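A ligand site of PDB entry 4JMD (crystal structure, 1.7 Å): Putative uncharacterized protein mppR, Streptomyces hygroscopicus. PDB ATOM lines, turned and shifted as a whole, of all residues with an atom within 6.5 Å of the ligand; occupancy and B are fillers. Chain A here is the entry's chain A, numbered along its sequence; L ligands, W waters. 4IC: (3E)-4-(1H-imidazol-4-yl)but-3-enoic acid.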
ATOM      1  N   TRP A  56      16.404 -20.895 -35.345  1.00  0.00           N
ATOM      2  CA  TRP A  56      16.685 -20.016 -34.234  1.00  0.00           C
ATOM      3  C   TRP A  56      17.958 -20.482 -33.538  1.00  0.00           C
ATOM      4  O   TRP A  56      18.187 -21.695 -33.352  1.00  0.00           O
ATOM      5  CB  TRP A  56      15.539 -19.961 -33.216  1.00  0.00           C
ATOM      6  CG  TRP A  56      14.154 -19.789 -33.833  1.00  0.00           C
ATOM      7  CD1 TRP A  56      13.685 -18.690 -34.494  1.00  0.00           C
ATOM      8  CD2 TRP A  56      13.060 -20.714 -33.785  1.00  0.00           C
ATOM      9  NE1 TRP A  56      12.372 -18.888 -34.882  1.00  0.00           N
ATOM     10  CE2 TRP A  56      11.971 -20.130 -34.455  1.00  0.00           C
ATOM     11  CE3 TRP A  56      12.909 -21.998 -33.244  1.00  0.00           C
ATOM     12  CZ2 TRP A  56      10.757 -20.768 -34.598  1.00  0.00           C
ATOM     13  CZ3 TRP A  56      11.685 -22.630 -33.394  1.00  0.00           C
ATOM     14  CH2 TRP A  56      10.623 -22.021 -34.069  1.00  0.00           C
ATOM     15  N   PHE A  58      20.451 -20.385 -30.175  1.00  0.00           N
ATOM     16  CA  PHE A  58      20.395 -20.285 -28.708  1.00  0.00           C
ATOM     17  C   PHE A  58      21.799 -20.302 -28.114  1.00  0.00           C
ATOM     18  O   PHE A  58      22.646 -21.116 -28.529  1.00  0.00           O
ATOM     19  CB  PHE A  58      19.612 -21.476 -28.139  1.00  0.00           C
ATOM     20  CG  PHE A  58      18.154 -21.461 -28.497  1.00  0.00           C
ATOM     21  CD1 PHE A  58      17.711 -22.009 -29.685  1.00  0.00           C
ATOM     22  CD2 PHE A  58      17.226 -20.867 -27.642  1.00  0.00           C
ATOM     23  CE1 PHE A  58      16.364 -21.947 -30.024  1.00  0.00           C
ATOM     24  CE2 PHE A  58      15.874 -20.827 -27.978  1.00  0.00           C
ATOM     25  CZ  PHE A  58      15.441 -21.381 -29.158  1.00  0.00           C
ATOM     26  N   ALA A  96      18.264 -22.961 -16.893  1.00  0.00           N
ATOM     27  CA  ALA A  96      19.082 -22.261 -17.863  1.00  0.00           C
ATOM     28  C   ALA A  96      18.638 -20.829 -18.065  1.00  0.00           C
ATOM     29  O   ALA A  96      17.439 -20.511 -17.906  1.00  0.00           O
ATOM     30  CB  ALA A  96      19.048 -23.018 -19.207  1.00  0.00           C
ATOM     31  N   TRP A  98      18.905 -18.037 -21.238  1.00  0.00           N
ATOM     32  CA  TRP A  98      19.180 -18.062 -22.654  1.00  0.00           C
ATOM     33  C   TRP A  98      19.160 -16.694 -23.281  1.00  0.00           C
ATOM     34  O   TRP A  98      18.404 -15.800 -22.835  1.00  0.00           O
ATOM     35  CB  TRP A  98      18.093 -18.855 -23.388  1.00  0.00           C
ATOM     36  CG  TRP A  98      17.963 -20.277 -22.991  1.00  0.00           C
ATOM     37  CD1 TRP A  98      16.999 -20.833 -22.183  1.00  0.00           C
ATOM     38  CD2 TRP A  98      18.794 -21.365 -23.423  1.00  0.00           C
ATOM     39  NE1 TRP A  98      17.206 -22.190 -22.075  1.00  0.00           N
ATOM     40  CE2 TRP A  98      18.294 -22.538 -22.828  1.00  0.00           C
ATOM     41  CE3 TRP A  98      19.913 -21.449 -24.248  1.00  0.00           C
ATOM     42  CZ2 TRP A  98      18.890 -23.788 -23.021  1.00  0.00           C
ATOM     43  CZ3 TRP A  98      20.500 -22.680 -24.456  1.00  0.00           C
ATOM     44  CH2 TRP A  98      19.985 -23.842 -23.845  1.00  0.00           C
ATOM     45  N   TRP A 100      18.516 -15.783 -27.453  1.00  0.00           N
ATOM     46  CA  TRP A 100      18.153 -16.411 -28.716  1.00  0.00           C
ATOM     47  C   TRP A 100      18.013 -15.346 -29.796  1.00  0.00           C
ATOM     48  O   TRP A 100      17.831 -14.142 -29.512  1.00  0.00           O
ATOM     49  CB  TRP A 100      16.841 -17.214 -28.611  1.00  0.00           C
ATOM     50  CG  TRP A 100      15.651 -16.354 -28.365  1.00  0.00           C
ATOM     51  CD1 TRP A 100      15.140 -15.957 -27.153  1.00  0.00           C
ATOM     52  CD2 TRP A 100      14.833 -15.724 -29.369  1.00  0.00           C
ATOM     53  NE1 TRP A 100      14.067 -15.120 -27.348  1.00  0.00           N
ATOM     54  CE2 TRP A 100      13.855 -14.968 -28.698  1.00  0.00           C
ATOM     55  CE3 TRP A 100      14.839 -15.739 -30.771  1.00  0.00           C
ATOM     56  CZ2 TRP A 100      12.880 -14.232 -29.379  1.00  0.00           C
ATOM     57  CZ3 TRP A 100      13.848 -14.989 -31.446  1.00  0.00           C
ATOM     58  CH2 TRP A 100      12.902 -14.254 -30.743  1.00  0.00           C
ATOM     59  N   PHE A 116      15.522 -15.145 -21.987  1.00  0.00           N
ATOM     60  CA  PHE A 116      14.550 -15.775 -21.108  1.00  0.00           C
ATOM     61  C   PHE A 116      15.223 -16.765 -20.172  1.00  0.00           C
ATOM     62  O   PHE A 116      16.345 -17.223 -20.435  1.00  0.00           O
ATOM     63  CB  PHE A 116      13.392 -16.471 -21.867  1.00  0.00           C
ATOM     64  CG  PHE A 116      13.783 -17.709 -22.654  1.00  0.00           C
ATOM     65  CD1 PHE A 116      14.368 -17.590 -23.909  1.00  0.00           C
ATOM     66  CD2 PHE A 116      13.458 -18.967 -22.186  1.00  0.00           C
ATOM     67  CE1 PHE A 116      14.679 -18.726 -24.655  1.00  0.00           C
ATOM     68  CE2 PHE A 116      13.732 -20.095 -22.917  1.00  0.00           C
ATOM     69  CZ  PHE A 116      14.344 -20.000 -24.160  1.00  0.00           C
ATOM     70  N   GLU A 118      14.593 -20.513 -17.918  1.00  0.00           N
ATOM     71  CA  GLU A 118      13.894 -21.784 -18.134  1.00  0.00           C
ATOM     72  C   GLU A 118      14.267 -22.802 -17.068  1.00  0.00           C
ATOM     73  O   GLU A 118      15.397 -22.825 -16.582  1.00  0.00           O
ATOM     74  CB  GLU A 118      14.312 -22.344 -19.499  1.00  0.00           C
ATOM     75  CG  GLU A 118      13.593 -23.603 -19.911  1.00  0.00           C
ATOM     76  CD  GLU A 118      14.120 -24.033 -21.283  1.00  0.00           C
ATOM     77  OE1 GLU A 118      13.317 -24.243 -22.180  1.00  0.00           O
ATOM     78  OE2 GLU A 118      15.354 -24.179 -21.397  1.00  0.00           O
ATOM     79  N   LEU A 120      13.538 -27.087 -16.649  1.00  0.00           N
ATOM     80  CA  LEU A 120      12.886 -28.250 -17.192  1.00  0.00           C
ATOM     81  C   LEU A 120      13.373 -29.539 -16.544  1.00  0.00           C
ATOM     82  O   LEU A 120      14.446 -29.612 -15.943  1.00  0.00           O
ATOM     83  CB  LEU A 120      13.030 -28.264 -18.711  1.00  0.00           C
ATOM     84  CG  LEU A 120      14.408 -28.144 -19.339  1.00  0.00           C
ATOM     85  CD1 LEU A 120      15.059 -29.494 -19.232  1.00  0.00           C
ATOM     86  CD2 LEU A 120      14.349 -27.673 -20.752  1.00  0.00           C
ATOM     87  N   VAL A 140       9.040 -21.351 -18.478  1.00  0.00           N
ATOM     88  CA  VAL A 140       9.810 -20.202 -18.933  1.00  0.00           C
ATOM     89  C   VAL A 140       9.185 -18.928 -18.400  1.00  0.00           C
ATOM     90  O   VAL A 140       8.077 -18.968 -17.862  1.00  0.00           O
ATOM     91  CB  VAL A 140       9.926 -20.081 -20.467  1.00  0.00           C
ATOM     92  CG1 VAL A 140      10.705 -21.259 -21.053  1.00  0.00           C
ATOM     93  CG2 VAL A 140       8.527 -19.966 -21.134  1.00  0.00           C
ATOM     94  N   VAL A 144       7.129 -15.229 -25.765  1.00  0.00           N
ATOM     95  CA  VAL A 144       7.520 -15.732 -27.076  1.00  0.00           C
ATOM     96  C   VAL A 144       8.104 -17.145 -26.943  1.00  0.00           C
ATOM     97  O   VAL A 144       7.687 -18.052 -27.641  1.00  0.00           O
ATOM     98  CB  VAL A 144       8.447 -14.767 -27.849  1.00  0.00           C
ATOM     99  CG1 VAL A 144       9.202 -15.472 -28.972  1.00  0.00           C
ATOM    100  CG2 VAL A 144       7.637 -13.599 -28.397  1.00  0.00           C
ATOM    101  N   PRO A 145       9.051 -17.344 -26.015  1.00  0.00           N
ATOM    102  CA  PRO A 145       9.543 -18.719 -25.872  1.00  0.00           C
ATOM    103  C   PRO A 145       8.447 -19.691 -25.459  1.00  0.00           C
ATOM    104  O   PRO A 145       8.490 -20.841 -25.904  1.00  0.00           O
ATOM    105  CB  PRO A 145      10.639 -18.580 -24.810  1.00  0.00           C
ATOM    106  CG  PRO A 145      11.140 -17.178 -24.979  1.00  0.00           C
ATOM    107  CD  PRO A 145       9.934 -16.353 -25.379  1.00  0.00           C
ATOM    108  N   MET A 146       7.516 -19.241 -24.631  1.00  0.00           N
ATOM    109  CA  MET A 146       6.450 -20.149 -24.209  1.00  0.00           C
ATOM    110  C   MET A 146       5.659 -20.684 -25.419  1.00  0.00           C
ATOM    111  O   MET A 146       5.491 -21.896 -25.583  1.00  0.00           O
ATOM    112  CB  MET A 146       5.518 -19.517 -23.193  1.00  0.00           C
ATOM    113  CG  MET A 146       4.455 -20.516 -22.728  1.00  0.00           C
ATOM    114  SD  MET A 146       3.392 -19.782 -21.476  1.00  0.00           S
ATOM    115  CE  MET A 146       2.729 -18.397 -22.385  1.00  0.00           C
ATOM    116  N   ARG A 148       6.470 -20.550 -28.623  1.00  0.00           N
ATOM    117  CA  ARG A 148       7.357 -21.255 -29.533  1.00  0.00           C
ATOM    118  C   ARG A 148       7.604 -22.666 -29.045  1.00  0.00           C
ATOM    119  O   ARG A 148       7.799 -23.585 -29.836  1.00  0.00           O
ATOM    120  CB  ARG A 148       8.693 -20.508 -29.660  1.00  0.00           C
ATOM    121  CG  ARG A 148       9.529 -20.922 -30.850  1.00  0.00           C
ATOM    122  CD  ARG A 148      10.674 -19.949 -31.107  1.00  0.00           C
ATOM    123  NE  ARG A 148      11.496 -19.735 -29.924  1.00  0.00           N
ATOM    124  CZ  ARG A 148      12.108 -18.586 -29.647  1.00  0.00           C
ATOM    125  NH1 ARG A 148      12.035 -17.568 -30.504  1.00  0.00           N
ATOM    126  NH2 ARG A 148      12.831 -18.461 -28.529  1.00  0.00           N
ATOM    127  N   GLY A 149       7.609 -22.860 -27.724  1.00  0.00           N
ATOM    128  CA  GLY A 149       7.749 -24.198 -27.182  1.00  0.00           C
ATOM    129  C   GLY A 149       6.618 -25.095 -27.640  1.00  0.00           C
ATOM    130  O   GLY A 149       6.850 -26.213 -28.078  1.00  0.00           O
ATOM    131  N   GLN A 152       6.921 -26.579 -31.034  1.00  0.00           N
ATOM    132  CA  GLN A 152       7.853 -27.711 -31.118  1.00  0.00           C
ATOM    133  C   GLN A 152       7.385 -28.917 -30.346  1.00  0.00           C
ATOM    134  O   GLN A 152       8.013 -29.971 -30.423  1.00  0.00           O
ATOM    135  CB  GLN A 152       9.201 -27.355 -30.532  1.00  0.00           C
ATOM    136  CG  GLN A 152       9.906 -26.142 -30.981  1.00  0.00           C
ATOM    137  CD  GLN A 152      10.883 -25.701 -29.882  1.00  0.00           C
ATOM    138  OE1 GLN A 152      11.727 -26.470 -29.413  1.00  0.00           O
ATOM    139  NE2 GLN A 152      10.736 -24.472 -29.434  1.00  0.00           N
ATOM    140  N   MET A 154       7.183 -28.747 -26.971  1.00  0.00           N
ATOM    141  CA  MET A 154       7.809 -28.651 -25.696  1.00  0.00           C
ATOM    142  C   MET A 154       6.862 -28.031 -24.693  1.00  0.00           C
ATOM    143  O   MET A 154       6.433 -26.898 -24.869  1.00  0.00           O
ATOM    144  CB  MET A 154       9.033 -27.807 -25.834  1.00  0.00           C
ATOM    145  CG  MET A 154       9.972 -28.135 -24.801  1.00  0.00           C
ATOM    146  SD  MET A 154      11.460 -27.269 -25.154  1.00  0.00           S
ATOM    147  CE  MET A 154      11.711 -26.822 -23.509  1.00  0.00           C
ATOM    148  N   LYS A 156       5.913 -26.136 -22.349  1.00  0.00           N
ATOM    149  CA  LYS A 156       6.229 -24.963 -21.511  1.00  0.00           C
ATOM    150  C   LYS A 156       4.999 -24.303 -20.864  1.00  0.00           C
ATOM    151  O   LYS A 156       3.978 -24.088 -21.516  1.00  0.00           O
ATOM    152  CB  LYS A 156       6.945 -23.916 -22.356  1.00  0.00           C
ATOM    153  CG  LYS A 156       8.331 -24.281 -22.884  1.00  0.00           C
ATOM    154  CD  LYS A 156       8.944 -23.160 -23.717  1.00  0.00           C
ATOM    155  CE  LYS A 156      10.290 -23.569 -24.341  1.00  0.00           C
ATOM    156  NZ  LYS A 156      10.671 -22.572 -25.336  1.00  0.00           N
ATOM    157  N   HIS A 211      21.782 -33.931 -21.626  1.00  0.00           N
ATOM    158  CA  HIS A 211      21.858 -32.685 -22.354  1.00  0.00           C
ATOM    159  C   HIS A 211      22.578 -32.862 -23.687  1.00  0.00           C
ATOM    160  O   HIS A 211      22.866 -31.866 -24.368  1.00  0.00           O
ATOM    161  CB  HIS A 211      22.578 -31.598 -21.535  1.00  0.00           C
ATOM    162  CG  HIS A 211      22.013 -30.228 -21.726  1.00  0.00           C
ATOM    163  ND1 HIS A 211      22.111 -29.530 -22.906  1.00  0.00           N
ATOM    164  CD2 HIS A 211      21.344 -29.424 -20.873  1.00  0.00           C
ATOM    165  CE1 HIS A 211      21.514 -28.358 -22.780  1.00  0.00           C
ATOM    166  NE2 HIS A 211      21.037 -28.264 -21.547  1.00  0.00           N
ATOM    167  N   LEU A 215      15.897 -34.435 -28.122  1.00  0.00           N
ATOM    168  CA  LEU A 215      14.639 -34.315 -27.370  1.00  0.00           C
ATOM    169  C   LEU A 215      13.443 -34.799 -28.202  1.00  0.00           C
ATOM    170  O   LEU A 215      13.255 -34.389 -29.351  1.00  0.00           O
ATOM    171  CB  LEU A 215      14.390 -32.863 -26.965  1.00  0.00           C
ATOM    172  CG  LEU A 215      15.476 -32.165 -26.137  1.00  0.00           C
ATOM    173  CD1 LEU A 215      15.019 -30.751 -25.772  1.00  0.00           C
ATOM    174  CD2 LEU A 215      15.798 -33.003 -24.921  1.00  0.00           C
ATOM    175  N   TYR A 281      26.076 -23.475 -23.126  1.00  0.00           N
ATOM    176  CA  TYR A 281      25.584 -24.356 -24.180  1.00  0.00           C
ATOM    177  C   TYR A 281      25.056 -23.528 -25.351  1.00  0.00           C
ATOM    178  O   TYR A 281      24.430 -22.500 -25.156  1.00  0.00           O
ATOM    179  CB  TYR A 281      24.436 -25.221 -23.631  1.00  0.00           C
ATOM    180  CG  TYR A 281      23.798 -26.150 -24.657  1.00  0.00           C
ATOM    181  CD1 TYR A 281      24.355 -27.368 -24.943  1.00  0.00           C
ATOM    182  CD2 TYR A 281      22.650 -25.776 -25.331  1.00  0.00           C
ATOM    183  CE1 TYR A 281      23.772 -28.237 -25.869  1.00  0.00           C
ATOM    184  CE2 TYR A 281      22.053 -26.615 -26.266  1.00  0.00           C
ATOM    185  CZ  TYR A 281      22.631 -27.852 -26.517  1.00  0.00           C
ATOM    186  OH  TYR A 281      22.062 -28.717 -27.432  1.00  0.00           O
ATOM    187  N   GLU A 283      23.126 -24.055 -29.454  1.00  0.00           N
ATOM    188  CA  GLU A 283      22.631 -24.927 -30.536  1.00  0.00           C
ATOM    189  C   GLU A 283      21.816 -24.066 -31.472  1.00  0.00           C
ATOM    190  O   GLU A 283      21.378 -22.972 -31.090  1.00  0.00           O
ATOM    191  CB  GLU A 283      21.752 -26.067 -29.995  1.00  0.00           C
ATOM    192  CG  GLU A 283      20.404 -25.601 -29.478  1.00  0.00           C
ATOM    193  CD  GLU A 283      19.460 -26.714 -28.987  1.00  0.00           C
ATOM    194  OE1 GLU A 283      18.256 -26.433 -28.915  1.00  0.00           O
ATOM    195  OE2 GLU A 283      19.909 -27.846 -28.695  1.00  0.00           O
ATOM    196  N   LEU A 285      18.308 -24.489 -33.723  1.00  0.00           N
ATOM    197  CA  LEU A 285      17.106 -25.305 -33.874  1.00  0.00           C
ATOM    198  C   LEU A 285      16.480 -25.013 -35.229  1.00  0.00           C
ATOM    199  O   LEU A 285      16.166 -23.877 -35.540  1.00  0.00           O
ATOM    200  CB  LEU A 285      16.145 -24.963 -32.741  1.00  0.00           C
ATOM    201  CG  LEU A 285      14.858 -25.747 -32.514  1.00  0.00           C
ATOM    202  CD1 LEU A 285      15.115 -27.222 -32.292  1.00  0.00           C
ATOM    203  CD2 LEU A 285      14.146 -25.127 -31.307  1.00  0.00           C
HETATM  204  O01 4IC L   1      12.408 -20.571 -26.880  1.00  0.00           O
HETATM  205  C02 4IC L   1      11.992 -21.721 -27.120  1.00  0.00           C
HETATM  206  O03 4IC L   1      11.738 -22.048 -28.301  1.00  0.00           O
HETATM  207  C04 4IC L   1      11.833 -22.676 -26.002  1.00  0.00           C
HETATM  208  C06 4IC L   1      12.936 -23.522 -25.495  1.00  0.00           C
HETATM  209  C07 4IC L   1      14.093 -23.577 -26.207  1.00  0.00           C
HETATM  210  C08 4IC L   1      15.142 -24.476 -25.682  1.00  0.00           C
HETATM  211  C09 4IC L   1      16.232 -24.991 -26.396  1.00  0.00           C
HETATM  212  N10 4IC L   1      16.925 -25.759 -25.524  1.00  0.00           N
HETATM  213  C11 4IC L   1      16.325 -25.714 -24.319  1.00  0.00           C
HETATM  214  N12 4IC L   1      15.232 -24.934 -24.415  1.00  0.00           N
HETATM  215  O   HOH W   1      18.780 -28.030 -25.060  1.00  0.00           O
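NZ of Lys 156 is bonded to C04 of the ligand.
An oxygen (O01) of the ligand is in salt-bridge range of the guanidinium group (NH2) of Arg 148.
The side-chain amide nitrogen (NE2) of Gln 152 is in hydrogen-bond range of an oxygen (O03) of the ligand.
The side-chain carboxylate (OE1) of Glu 118 lies close to a nitrogen (N12) of the ligand (3.0 Å).
NZ of Lys 156 lies within hydrogen-bond range of O of Pro 145 (2.8 Å).
The backbone carbonyl oxygen of Arg 148 lies within hydrogen-bond range of the side-chain amide nitrogen of Gln 152 (3.1 Å).
The side-chain carboxylate (OE2) of Glu 118 sits at hydrogen-bond distance from the indole nitrogen (NE1) of Trp 98 (2.8 Å).
The backbone carbonyl oxygen (O) of Ala 96 sits at hydrogen-bond distance from the backbone NH (N) of Glu 118.
O of Phe 116 lies within hydrogen-bond range of N of Trp 98 (2.8 Å).
The backbone NH of Phe 58 sits at hydrogen-bond distance from the backbone carbonyl oxygen of Glu 283.
The side-chain carboxylate (OE2) of Glu 283 is in hydrogen-bond range of the side-chain hydroxyl (OH) of Tyr 281.
Phe 58 touches the ligand.
Trp 98 touches the ligand (CZ2 to C11, 3.5 Å).
Phe 116 touches the ligand (CZ to O01, 3.4 Å).
CB of Pro 145 touches O01 of the ligand, 3.4 Å away.
Glu 283 touches the ligand (OE1 to C09, 3.5 Å).
Hydrophobic or aromatic side chains within 4 Å of the ligand: Phe 58, Trp 98, Phe 116 and Pro 145.
Within 4 Å of the ligand: Phe 58, Trp 98, Phe 116, Glu 118, Pro 145, Arg 148, Gln 152, Lys 156 and Glu 283.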
